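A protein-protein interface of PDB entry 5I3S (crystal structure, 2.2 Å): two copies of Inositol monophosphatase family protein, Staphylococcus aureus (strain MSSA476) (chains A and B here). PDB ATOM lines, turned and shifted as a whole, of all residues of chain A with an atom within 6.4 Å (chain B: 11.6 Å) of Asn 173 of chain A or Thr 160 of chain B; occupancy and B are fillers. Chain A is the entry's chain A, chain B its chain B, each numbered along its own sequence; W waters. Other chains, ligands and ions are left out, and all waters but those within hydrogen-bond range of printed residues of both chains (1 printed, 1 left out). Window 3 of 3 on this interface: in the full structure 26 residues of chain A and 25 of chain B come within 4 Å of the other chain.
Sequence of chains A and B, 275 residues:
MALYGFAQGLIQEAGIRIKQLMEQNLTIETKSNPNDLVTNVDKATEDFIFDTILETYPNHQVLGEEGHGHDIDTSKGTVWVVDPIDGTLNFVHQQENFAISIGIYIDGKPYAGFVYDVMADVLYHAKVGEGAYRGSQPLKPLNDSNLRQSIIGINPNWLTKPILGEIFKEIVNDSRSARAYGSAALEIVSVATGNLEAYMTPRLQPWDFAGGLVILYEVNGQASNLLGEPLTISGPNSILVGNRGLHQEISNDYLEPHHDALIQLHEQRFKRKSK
The side-chain amide oxygen of Asn 173 of chain A sits close to the side-chain hydroxyl of Thr 160 of chain B (3.4 Å).
O of Lys 169 of chain A sits close to OD1 of Asn 173 of chain A.
The backbone carbonyl oxygen (O) of Val 172 of chain A sits at hydrogen-bond distance from the side-chain hydroxyl (OG) of Ser 175 of chain A (2.9 Å).
ND2 of Asn 155 of chain B lies close to ND2 of Asn 157 of chain B (2.9 Å).
The backbone carbonyl oxygen (O) of Asn 157 of chain B lies within hydrogen-bond range of the side-chain hydroxyl (OG1) of Thr 160 of chain B (2.7 Å).
Among the printed residues, pairs that only touch across the chains: Leu 159 of chain A with Pro 156 of chain B, Leu 159 of chain A with Thr 160 of chain B, Lys 169 of chain A with Leu 159 of chain B, Lys 169 of chain A with Thr 160 of chain B, Val 172 of chain A with Asn 157 of chain B, Val 172 of chain A with Thr 160 of chain B and Arg 176 of chain A with Leu 89 of chain B.
Of the printed residues of chain B, Leu 159 of chain A touches Pro 156 and Thr 160.
No residue of chain B comes within 4 Å of Ile 171 of chain A.
Of chain B, only Asn 157 (3.5 Å) and Thr 160 (3.9 Å) come within 4 Å of Val 172 of chain A.
Asn 173 of chain A touches just one residue of chain B: Thr 160 (3.3 Å).
No residue of chain B comes within 4 Å of Asp 174 of chain A.
No residue of chain B comes within 4 Å of Ser 175 of chain A.
Of the printed residues of chain B, Arg 176 of chain A touches Leu 89 (3.7 Å).
Of the printed residues of chain A, Leu 89 of chain B touches Arg 176.
Printed residues of chain A within 4 Å of Pro 156 of chain B: Leu 159 (3.5 Å).
Printed residues of chain A within 4 Å of Leu 159 of chain B: Lys 169 (3.1 Å).
Of the printed residues of chain A, Thr 160 of chain B touches Leu 159, Lys 169, Val 172 and Asn 173.
Gly 165 of chain B touches none of the printed residues of chain A.
Lys 169 of chain B touches none of the printed residues of chain A.
The nearest printed residue of chain A that does not touch Leu 89 of chain B is Ser 175 of chain A (7.3 Å).
Hydrophobic or aromatic side chains of chain A that line the printed part of chain B: Leu 159 and Val 172.
Hydrophobic or aromatic side chains of chain B that line the printed part of chain A: Leu 89.
Lys 169 of chain A touches Leu 159 of chain B, but with the chains exchanged Leu 159 of chain A does not touch Lys 169 of chain B (6.9 Å).
Positions printed for both chains: 159, 168, 169, 170 and 172.
Water W1 lies within hydrogen-bond range of OG of Ser 175 of chain A (2.5 Å), O of Val 172 of chain A (2.6 Å) and ND2 of Asn 157 of chain B (3.3 Å).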
ATOM      1  N   LEU A 159      20.211   0.623  21.811  1.00  0.00           N
ATOM      2  CA  LEU A 159      19.061  -0.255  21.626  1.00  0.00           C
ATOM      3  C   LEU A 159      17.998   0.296  20.683  1.00  0.00           C
ATOM      4  O   LEU A 159      17.101  -0.465  20.300  1.00  0.00           O
ATOM      5  CB  LEU A 159      18.438  -0.660  22.966  1.00  0.00           C
ATOM      6  CG  LEU A 159      19.267  -1.663  23.762  1.00  0.00           C
ATOM      7  CD1 LEU A 159      20.446  -1.011  24.466  1.00  0.00           C
ATOM      8  CD2 LEU A 159      18.395  -2.297  24.800  1.00  0.00           C
ATOM      9  N   PHE A 168      21.821  -6.136  20.149  1.00  0.00           N
ATOM     10  CA  PHE A 168      22.032  -5.883  21.593  1.00  0.00           C
ATOM     11  C   PHE A 168      20.825  -6.246  22.508  1.00  0.00           C
ATOM     12  O   PHE A 168      21.006  -6.483  23.725  1.00  0.00           O
ATOM     13  CB  PHE A 168      22.504  -4.440  21.882  1.00  0.00           C
ATOM     14  CG  PHE A 168      23.956  -4.139  21.525  1.00  0.00           C
ATOM     15  CD1 PHE A 168      24.994  -4.976  21.897  1.00  0.00           C
ATOM     16  CD2 PHE A 168      24.290  -2.912  20.928  1.00  0.00           C
ATOM     17  CE1 PHE A 168      26.323  -4.635  21.627  1.00  0.00           C
ATOM     18  CE2 PHE A 168      25.612  -2.578  20.648  1.00  0.00           C
ATOM     19  CZ  PHE A 168      26.622  -3.447  20.986  1.00  0.00           C
ATOM     20  N   LYS A 169      19.607  -6.332  21.951  1.00  0.00           N
ATOM     21  CA  LYS A 169      18.405  -6.626  22.765  1.00  0.00           C
ATOM     22  C   LYS A 169      18.470  -7.950  23.490  1.00  0.00           C
ATOM     23  O   LYS A 169      18.089  -8.025  24.643  1.00  0.00           O
ATOM     24  CB  LYS A 169      17.105  -6.587  21.950  1.00  0.00           C
ATOM     25  CG  LYS A 169      16.218  -5.375  22.250  1.00  0.00           C
ATOM     26  CD  LYS A 169      16.390  -4.203  21.288  1.00  0.00           C
ATOM     27  CE  LYS A 169      15.158  -3.324  21.225  1.00  0.00           C
ATOM     28  NZ  LYS A 169      14.182  -3.915  20.275  1.00  0.00           N
ATOM     29  N   GLU A 170      18.953  -8.988  22.816  1.00  0.00           N
ATOM     30  CA  GLU A 170      19.041 -10.320  23.401  1.00  0.00           C
ATOM     31  C   GLU A 170      20.045 -10.319  24.559  1.00  0.00           C
ATOM     32  O   GLU A 170      19.762 -10.828  25.631  1.00  0.00           O
ATOM     33  CB  GLU A 170      19.327 -11.405  22.316  1.00  0.00           C
ATOM     34  CG  GLU A 170      18.067 -11.906  21.569  1.00  0.00           C
ATOM     35  N   ILE A 171      21.184  -9.657  24.395  1.00  0.00           N
ATOM     36  CA  ILE A 171      22.158  -9.686  25.444  1.00  0.00           C
ATOM     37  C   ILE A 171      21.644  -8.867  26.665  1.00  0.00           C
ATOM     38  O   ILE A 171      21.872  -9.260  27.802  1.00  0.00           O
ATOM     39  CB  ILE A 171      23.607  -9.387  24.981  1.00  0.00           C
ATOM     40  CG1 ILE A 171      24.194  -8.187  25.640  1.00  0.00           C
ATOM     41  CG2 ILE A 171      23.815  -9.325  23.469  1.00  0.00           C
ATOM     42  CD1 ILE A 171      24.935  -8.600  26.886  1.00  0.00           C
ATOM     43  N   VAL A 172      20.904  -7.793  26.426  1.00  0.00           N
ATOM     44  CA  VAL A 172      20.294  -7.062  27.504  1.00  0.00           C
ATOM     45  C   VAL A 172      19.216  -7.919  28.206  1.00  0.00           C
ATOM     46  O   VAL A 172      19.097  -7.935  29.439  1.00  0.00           O
ATOM     47  CB  VAL A 172      19.681  -5.759  26.993  1.00  0.00           C
ATOM     48  CG1 VAL A 172      18.926  -5.052  28.102  1.00  0.00           C
ATOM     49  CG2 VAL A 172      20.783  -4.853  26.486  1.00  0.00           C
ATOM     50  N   ASN A 173      18.461  -8.644  27.393  1.00  0.00           N
ATOM     51  CA  ASN A 173      17.421  -9.492  27.886  1.00  0.00           C
ATOM     52  C   ASN A 173      17.942 -10.584  28.797  1.00  0.00           C
ATOM     53  O   ASN A 173      17.318 -10.877  29.811  1.00  0.00           O
ATOM     54  CB  ASN A 173      16.624 -10.113  26.757  1.00  0.00           C
ATOM     55  CG  ASN A 173      15.232  -9.585  26.730  1.00  0.00           C
ATOM     56  OD1 ASN A 173      14.956  -8.546  26.085  1.00  0.00           O
ATOM     57  ND2 ASN A 173      14.332 -10.247  27.516  1.00  0.00           N
ATOM     58  N   ASP A 174      19.067 -11.184  28.444  1.00  0.00           N
ATOM     59  CA  ASP A 174      19.559 -12.266  29.269  1.00  0.00           C
ATOM     60  C   ASP A 174      20.300 -11.741  30.485  1.00  0.00           C
ATOM     61  O   ASP A 174      20.212 -12.352  31.541  1.00  0.00           O
ATOM     62  CB  ASP A 174      20.333 -13.288  28.440  1.00  0.00           C
ATOM     63  CG  ASP A 174      19.387 -14.040  27.472  1.00  0.00           C
ATOM     64  OD1 ASP A 174      18.321 -14.568  27.917  1.00  0.00           O
ATOM     65  OD2 ASP A 174      19.665 -14.086  26.260  1.00  0.00           O
ATOM     66  N   SER A 175      20.974 -10.600  30.370  1.00  0.00           N
ATOM     67  CA  SER A 175      21.674 -10.064  31.546  1.00  0.00           C
ATOM     68  C   SER A 175      20.677  -9.787  32.677  1.00  0.00           C
ATOM     69  O   SER A 175      19.447  -9.692  32.482  1.00  0.00           O
ATOM     70  CB  SER A 175      22.506  -8.833  31.225  1.00  0.00           C
ATOM     71  OG  SER A 175      21.822  -7.984  30.346  1.00  0.00           O
ATOM     72  N   ARG A 176      21.219  -9.754  33.873  1.00  0.00           N
ATOM     73  CA  ARG A 176      20.428  -9.509  35.069  1.00  0.00           C
ATOM     74  C   ARG A 176      19.957  -8.077  35.082  1.00  0.00           C
ATOM     75  O   ARG A 176      18.794  -7.806  35.432  1.00  0.00           O
ATOM     76  CB  ARG A 176      21.274  -9.782  36.302  1.00  0.00           C
ATOM     77  CG  ARG A 176      20.502  -9.843  37.589  1.00  0.00           C
ATOM     78  CD  ARG A 176      19.607 -11.079  37.691  1.00  0.00           C
ATOM     79  NE  ARG A 176      18.926 -11.082  38.977  1.00  0.00           N
ATOM     80  CZ  ARG A 176      17.875 -10.307  39.294  1.00  0.00           C
ATOM     81  NH1 ARG A 176      17.326  -9.452  38.414  1.00  0.00           N
ATOM     82  NH2 ARG A 176      17.361 -10.389  40.526  1.00  0.00           N
ATOM     83  N   LEU B  89      20.672  -4.968  43.409  1.00  0.00           N
ATOM     84  CA  LEU B  89      21.698  -5.468  42.472  1.00  0.00           C
ATOM     85  C   LEU B  89      23.006  -4.722  42.584  1.00  0.00           C
ATOM     86  O   LEU B  89      24.091  -5.341  42.483  1.00  0.00           O
ATOM     87  CB  LEU B  89      21.260  -5.415  40.996  1.00  0.00           C
ATOM     88  CG  LEU B  89      20.458  -6.636  40.574  1.00  0.00           C
ATOM     89  CD1 LEU B  89      20.046  -6.458  39.111  1.00  0.00           C
ATOM     90  CD2 LEU B  89      21.258  -7.943  40.785  1.00  0.00           C
ATOM     91  N   ILE B 154      17.157   6.197  32.159  1.00  0.00           N
ATOM     92  CA  ILE B 154      16.228   5.140  31.817  1.00  0.00           C
ATOM     93  C   ILE B 154      17.044   3.860  31.611  1.00  0.00           C
ATOM     94  O   ILE B 154      18.024   3.859  30.925  1.00  0.00           O
ATOM     95  CB  ILE B 154      15.450   5.500  30.553  1.00  0.00           C
ATOM     96  CG1 ILE B 154      14.451   4.399  30.222  1.00  0.00           C
ATOM     97  CG2 ILE B 154      16.396   5.745  29.359  1.00  0.00           C
ATOM     98  CD1 ILE B 154      13.740   4.691  28.926  1.00  0.00           C
ATOM     99  N   ASN B 155      16.605   2.760  32.161  1.00  0.00           N
ATOM    100  CA  ASN B 155      17.350   1.503  32.041  1.00  0.00           C
ATOM    101  C   ASN B 155      17.180   0.941  30.626  1.00  0.00           C
ATOM    102  O   ASN B 155      16.085   0.947  30.116  1.00  0.00           O
ATOM    103  CB  ASN B 155      16.794   0.544  33.080  1.00  0.00           C
ATOM    104  CG  ASN B 155      17.694  -0.661  33.366  1.00  0.00           C
ATOM    105  OD1 ASN B 155      18.142  -0.851  34.481  1.00  0.00           O
ATOM    106  ND2 ASN B 155      17.883  -1.473  32.412  1.00  0.00           N
ATOM    107  N   PRO B 156      18.264   0.486  29.968  1.00  0.00           N
ATOM    108  CA  PRO B 156      18.167  -0.181  28.687  1.00  0.00           C
ATOM    109  C   PRO B 156      17.118  -1.274  28.583  1.00  0.00           C
ATOM    110  O   PRO B 156      16.468  -1.432  27.570  1.00  0.00           O
ATOM    111  CB  PRO B 156      19.567  -0.794  28.543  1.00  0.00           C
ATOM    112  CG  PRO B 156      20.464   0.274  29.134  1.00  0.00           C
ATOM    113  CD  PRO B 156      19.666   0.709  30.362  1.00  0.00           C
ATOM    114  N   ASN B 157      16.952  -2.086  29.595  1.00  0.00           N
ATOM    115  CA  ASN B 157      15.820  -3.050  29.599  1.00  0.00           C
ATOM    116  C   ASN B 157      14.482  -2.577  29.128  1.00  0.00           C
ATOM    117  O   ASN B 157      13.796  -3.289  28.407  1.00  0.00           O
ATOM    118  CB  ASN B 157      15.625  -3.666  30.939  1.00  0.00           C
ATOM    119  CG  ASN B 157      16.636  -4.700  31.184  1.00  0.00           C
ATOM    120  OD1 ASN B 157      16.530  -5.809  30.641  1.00  0.00           O
ATOM    121  ND2 ASN B 157      17.683  -4.341  31.911  1.00  0.00           N
ATOM    122  N   TRP B 158      14.076  -1.381  29.497  1.00  0.00           N
ATOM    123  CA  TRP B 158      12.727  -0.960  29.099  1.00  0.00           C
ATOM    124  C   TRP B 158      12.593  -0.770  27.582  1.00  0.00           C
ATOM    125  O   TRP B 158      11.498  -0.881  27.030  1.00  0.00           O
ATOM    126  CB  TRP B 158      12.352   0.274  29.851  1.00  0.00           C
ATOM    127  CG  TRP B 158      12.490   0.134  31.299  1.00  0.00           C
ATOM    128  CD1 TRP B 158      13.249   0.912  32.112  1.00  0.00           C
ATOM    129  CD2 TRP B 158      11.853  -0.836  32.153  1.00  0.00           C
ATOM    130  NE1 TRP B 158      13.086   0.540  33.416  1.00  0.00           N
ATOM    131  CE2 TRP B 158      12.246  -0.542  33.473  1.00  0.00           C
ATOM    132  CE3 TRP B 158      10.982  -1.908  31.935  1.00  0.00           C
ATOM    133  CZ2 TRP B 158      11.833  -1.308  34.566  1.00  0.00           C
ATOM    134  CZ3 TRP B 158      10.534  -2.635  33.028  1.00  0.00           C
ATOM    135  CH2 TRP B 158      10.986  -2.343  34.328  1.00  0.00           C
ATOM    136  N   LEU B 159      13.717  -0.532  26.912  1.00  0.00           N
ATOM    137  CA  LEU B 159      13.758  -0.502  25.453  1.00  0.00           C
ATOM    138  C   LEU B 159      13.650  -1.892  24.743  1.00  0.00           C
ATOM    139  O   LEU B 159      13.581  -1.944  23.541  1.00  0.00           O
ATOM    140  CB  LEU B 159      14.983   0.266  24.959  1.00  0.00           C
ATOM    141  CG  LEU B 159      14.796   1.796  24.890  1.00  0.00           C
ATOM    142  CD1 LEU B 159      14.318   2.431  26.178  1.00  0.00           C
ATOM    143  CD2 LEU B 159      16.112   2.429  24.509  1.00  0.00           C
ATOM    144  N   THR B 160      13.643  -2.999  25.481  1.00  0.00           N
ATOM    145  CA  THR B 160      13.530  -4.324  24.875  1.00  0.00           C
ATOM    146  C   THR B 160      12.071  -4.780  24.771  1.00  0.00           C
ATOM    147  O   THR B 160      11.767  -5.646  23.990  1.00  0.00           O
ATOM    148  CB  THR B 160      14.317  -5.368  25.681  1.00  0.00           C
ATOM    149  OG1 THR B 160      13.729  -5.545  26.980  1.00  0.00           O
ATOM    150  CG2 THR B 160      15.779  -4.944  25.833  1.00  0.00           C
ATOM    151  N   LYS B 161      11.183  -4.177  25.550  1.00  0.00           N
ATOM    152  CA  LYS B 161       9.838  -4.693  25.751  1.00  0.00           C
ATOM    153  C   LYS B 161       8.998  -4.313  24.520  1.00  0.00           C
ATOM    154  O   LYS B 161       9.330  -3.331  23.842  1.00  0.00           O
ATOM    155  CB  LYS B 161       9.239  -4.122  27.055  1.00  0.00           C
ATOM    156  CG  LYS B 161      10.121  -4.201  28.314  1.00  0.00           C
ATOM    157  CD  LYS B 161      10.408  -5.624  28.761  1.00  0.00           C
ATOM    158  CE  LYS B 161      11.551  -5.667  29.756  1.00  0.00           C
ATOM    159  NZ  LYS B 161      11.702  -7.039  30.265  1.00  0.00           N
ATOM    160  N   PRO B 162       7.924  -5.086  24.220  1.00  0.00           N
ATOM    161  CA  PRO B 162       7.290  -4.932  22.902  1.00  0.00           C
ATOM    162  C   PRO B 162       6.629  -3.550  22.718  1.00  0.00           C
ATOM    163  O   PRO B 162       6.935  -2.825  21.743  1.00  0.00           O
ATOM    164  CB  PRO B 162       6.267  -6.080  22.862  1.00  0.00           C
ATOM    165  CG  PRO B 162       5.963  -6.407  24.289  1.00  0.00           C
ATOM    166  CD  PRO B 162       7.115  -5.923  25.133  1.00  0.00           C
ATOM    167  N   ILE B 163       5.791  -3.169  23.674  1.00  0.00           N
ATOM    168  CA  ILE B 163       4.976  -1.973  23.544  1.00  0.00           C
ATOM    169  C   ILE B 163       5.690  -0.777  24.173  1.00  0.00           C
ATOM    170  O   ILE B 163       5.631   0.331  23.628  1.00  0.00           O
ATOM    171  CB  ILE B 163       3.582  -2.198  24.168  1.00  0.00           C
ATOM    172  CG1 ILE B 163       2.886  -3.409  23.504  1.00  0.00           C
ATOM    173  CG2 ILE B 163       2.700  -0.945  24.052  1.00  0.00           C
ATOM    174  CD1 ILE B 163       2.291  -3.141  22.129  1.00  0.00           C
ATOM    175  N   LEU B 164       6.354  -1.013  25.310  1.00  0.00           N
ATOM    176  CA  LEU B 164       7.216  -0.021  25.979  1.00  0.00           C
ATOM    177  C   LEU B 164       8.386   0.467  25.119  1.00  0.00           C
ATOM    178  O   LEU B 164       8.665   1.663  25.065  1.00  0.00           O
ATOM    179  CB  LEU B 164       7.824  -0.600  27.287  1.00  0.00           C
ATOM    180  CG  LEU B 164       7.165  -0.482  28.656  1.00  0.00           C
ATOM    181  CD1 LEU B 164       6.407   0.835  28.779  1.00  0.00           C
ATOM    182  CD2 LEU B 164       6.267  -1.678  28.910  1.00  0.00           C
ATOM    183  N   GLY B 165       9.087  -0.466  24.489  1.00  0.00           N
ATOM    184  CA  GLY B 165      10.270  -0.146  23.714  1.00  0.00           C
ATOM    185  C   GLY B 165       9.965   0.905  22.674  1.00  0.00           C
ATOM    186  O   GLY B 165      10.763   1.818  22.460  1.00  0.00           O
ATOM    187  N   GLU B 166       8.807   0.791  22.030  1.00  0.00           N
ATOM    188  CA  GLU B 166       8.390   1.791  21.067  1.00  0.00           C
ATOM    189  C   GLU B 166       7.963   3.098  21.816  1.00  0.00           C
ATOM    190  O   GLU B 166       8.370   4.190  21.437  1.00  0.00           O
ATOM    191  CB  GLU B 166       7.305   1.254  20.089  1.00  0.00           C
ATOM    192  CG  GLU B 166       7.584  -0.068  19.317  1.00  0.00           C
ATOM    193  CD  GLU B 166       8.973  -0.239  18.628  1.00  0.00           C
ATOM    194  OE1 GLU B 166       9.403  -1.421  18.461  1.00  0.00           O
ATOM    195  OE2 GLU B 166       9.647   0.752  18.228  1.00  0.00           O
ATOM    196  N   ILE B 167       7.213   2.979  22.911  1.00  0.00           N
ATOM    197  CA  ILE B 167       6.788   4.147  23.686  1.00  0.00           C
ATOM    198  C   ILE B 167       7.941   5.039  24.151  1.00  0.00           C
ATOM    199  O   ILE B 167       7.736   6.235  24.233  1.00  0.00           O
ATOM    200  CB  ILE B 167       5.907   3.755  24.904  1.00  0.00           C
ATOM    201  N   PHE B 168       9.121   4.473  24.448  1.00  0.00           N
ATOM    202  CA  PHE B 168      10.313   5.249  24.911  1.00  0.00           C
ATOM    203  C   PHE B 168      11.325   5.637  23.820  1.00  0.00           C
ATOM    204  O   PHE B 168      12.107   6.587  24.010  1.00  0.00           O
ATOM    205  CB  PHE B 168      11.079   4.479  26.008  1.00  0.00           C
ATOM    206  CG  PHE B 168      10.377   4.431  27.341  1.00  0.00           C
ATOM    207  CD1 PHE B 168      10.048   5.607  28.010  1.00  0.00           C
ATOM    208  CD2 PHE B 168      10.090   3.210  27.946  1.00  0.00           C
ATOM    209  CE1 PHE B 168       9.403   5.570  29.238  1.00  0.00           C
ATOM    210  CE2 PHE B 168       9.469   3.149  29.189  1.00  0.00           C
ATOM    211  CZ  PHE B 168       9.121   4.334  29.838  1.00  0.00           C
ATOM    212  N   LYS B 169      11.328   4.872  22.721  1.00  0.00           N
ATOM    213  CA  LYS B 169      12.276   5.012  21.591  1.00  0.00           C
ATOM    214  C   LYS B 169      12.521   6.436  21.182  1.00  0.00           C
ATOM    215  O   LYS B 169      13.649   6.906  21.114  1.00  0.00           O
ATOM    216  CB  LYS B 169      11.706   4.254  20.387  1.00  0.00           C
ATOM    217  CG  LYS B 169      12.371   4.425  19.025  1.00  0.00           C
ATOM    218  CD  LYS B 169      11.694   3.492  18.013  1.00  0.00           C
ATOM    219  CE  LYS B 169      11.686   4.073  16.602  1.00  0.00           C
ATOM    220  NZ  LYS B 169      13.084   4.431  16.182  1.00  0.00           N
ATOM    221  N   GLU B 170      11.440   7.128  20.913  1.00  0.00           N
ATOM    222  CA  GLU B 170      11.526   8.447  20.341  1.00  0.00           C
ATOM    223  C   GLU B 170      12.116   9.442  21.392  1.00  0.00           C
ATOM    224  O   GLU B 170      12.956  10.270  21.062  1.00  0.00           O
ATOM    225  CB  GLU B 170      10.160   8.827  19.678  1.00  0.00           C
ATOM    226  CG  GLU B 170       9.856   7.981  18.411  1.00  0.00           C
ATOM    227  N   VAL B 172      14.340   8.627  23.841  1.00  0.00           N
ATOM    228  CA  VAL B 172      15.799   8.375  23.862  1.00  0.00           C
ATOM    229  C   VAL B 172      16.476   9.053  22.648  1.00  0.00           C
ATOM    230  O   VAL B 172      17.502   9.709  22.804  1.00  0.00           O
ATOM    231  CB  VAL B 172      16.179   6.857  23.971  1.00  0.00           C
ATOM    232  CG1 VAL B 172      17.696   6.649  23.905  1.00  0.00           C
ATOM    233  CG2 VAL B 172      15.617   6.278  25.266  1.00  0.00           C
ATOM    234  N   PRO B 202       8.651   2.492  33.793  1.00  0.00           N
ATOM    235  CA  PRO B 202       7.265   2.075  33.732  1.00  0.00           C
ATOM    236  C   PRO B 202       6.720   1.432  34.999  1.00  0.00           C
ATOM    237  O   PRO B 202       5.503   1.331  35.116  1.00  0.00           O
ATOM    238  CB  PRO B 202       7.265   1.031  32.605  1.00  0.00           C
ATOM    239  CG  PRO B 202       8.662   0.462  32.652  1.00  0.00           C
ATOM    240  CD  PRO B 202       9.496   1.686  32.898  1.00  0.00           C
ATOM    241  N   LEU B 265      -1.538  -0.792  29.368  1.00  0.00           N
ATOM    242  CA  LEU B 265      -0.427  -1.319  30.164  1.00  0.00           C
ATOM    243  C   LEU B 265      -0.637  -1.079  31.658  1.00  0.00           C
ATOM    244  O   LEU B 265      -0.439  -2.001  32.459  1.00  0.00           O
ATOM    245  CB  LEU B 265       0.914  -0.715  29.727  1.00  0.00           C
ATOM    246  CG  LEU B 265       1.567  -1.283  28.462  1.00  0.00           C
ATOM    247  CD1 LEU B 265       2.716  -0.369  28.044  1.00  0.00           C
ATOM    248  CD2 LEU B 265       2.046  -2.715  28.680  1.00  0.00           C
HETATM  249  O   HOH W   1      20.201  -6.272  31.170  1.00  0.00           O
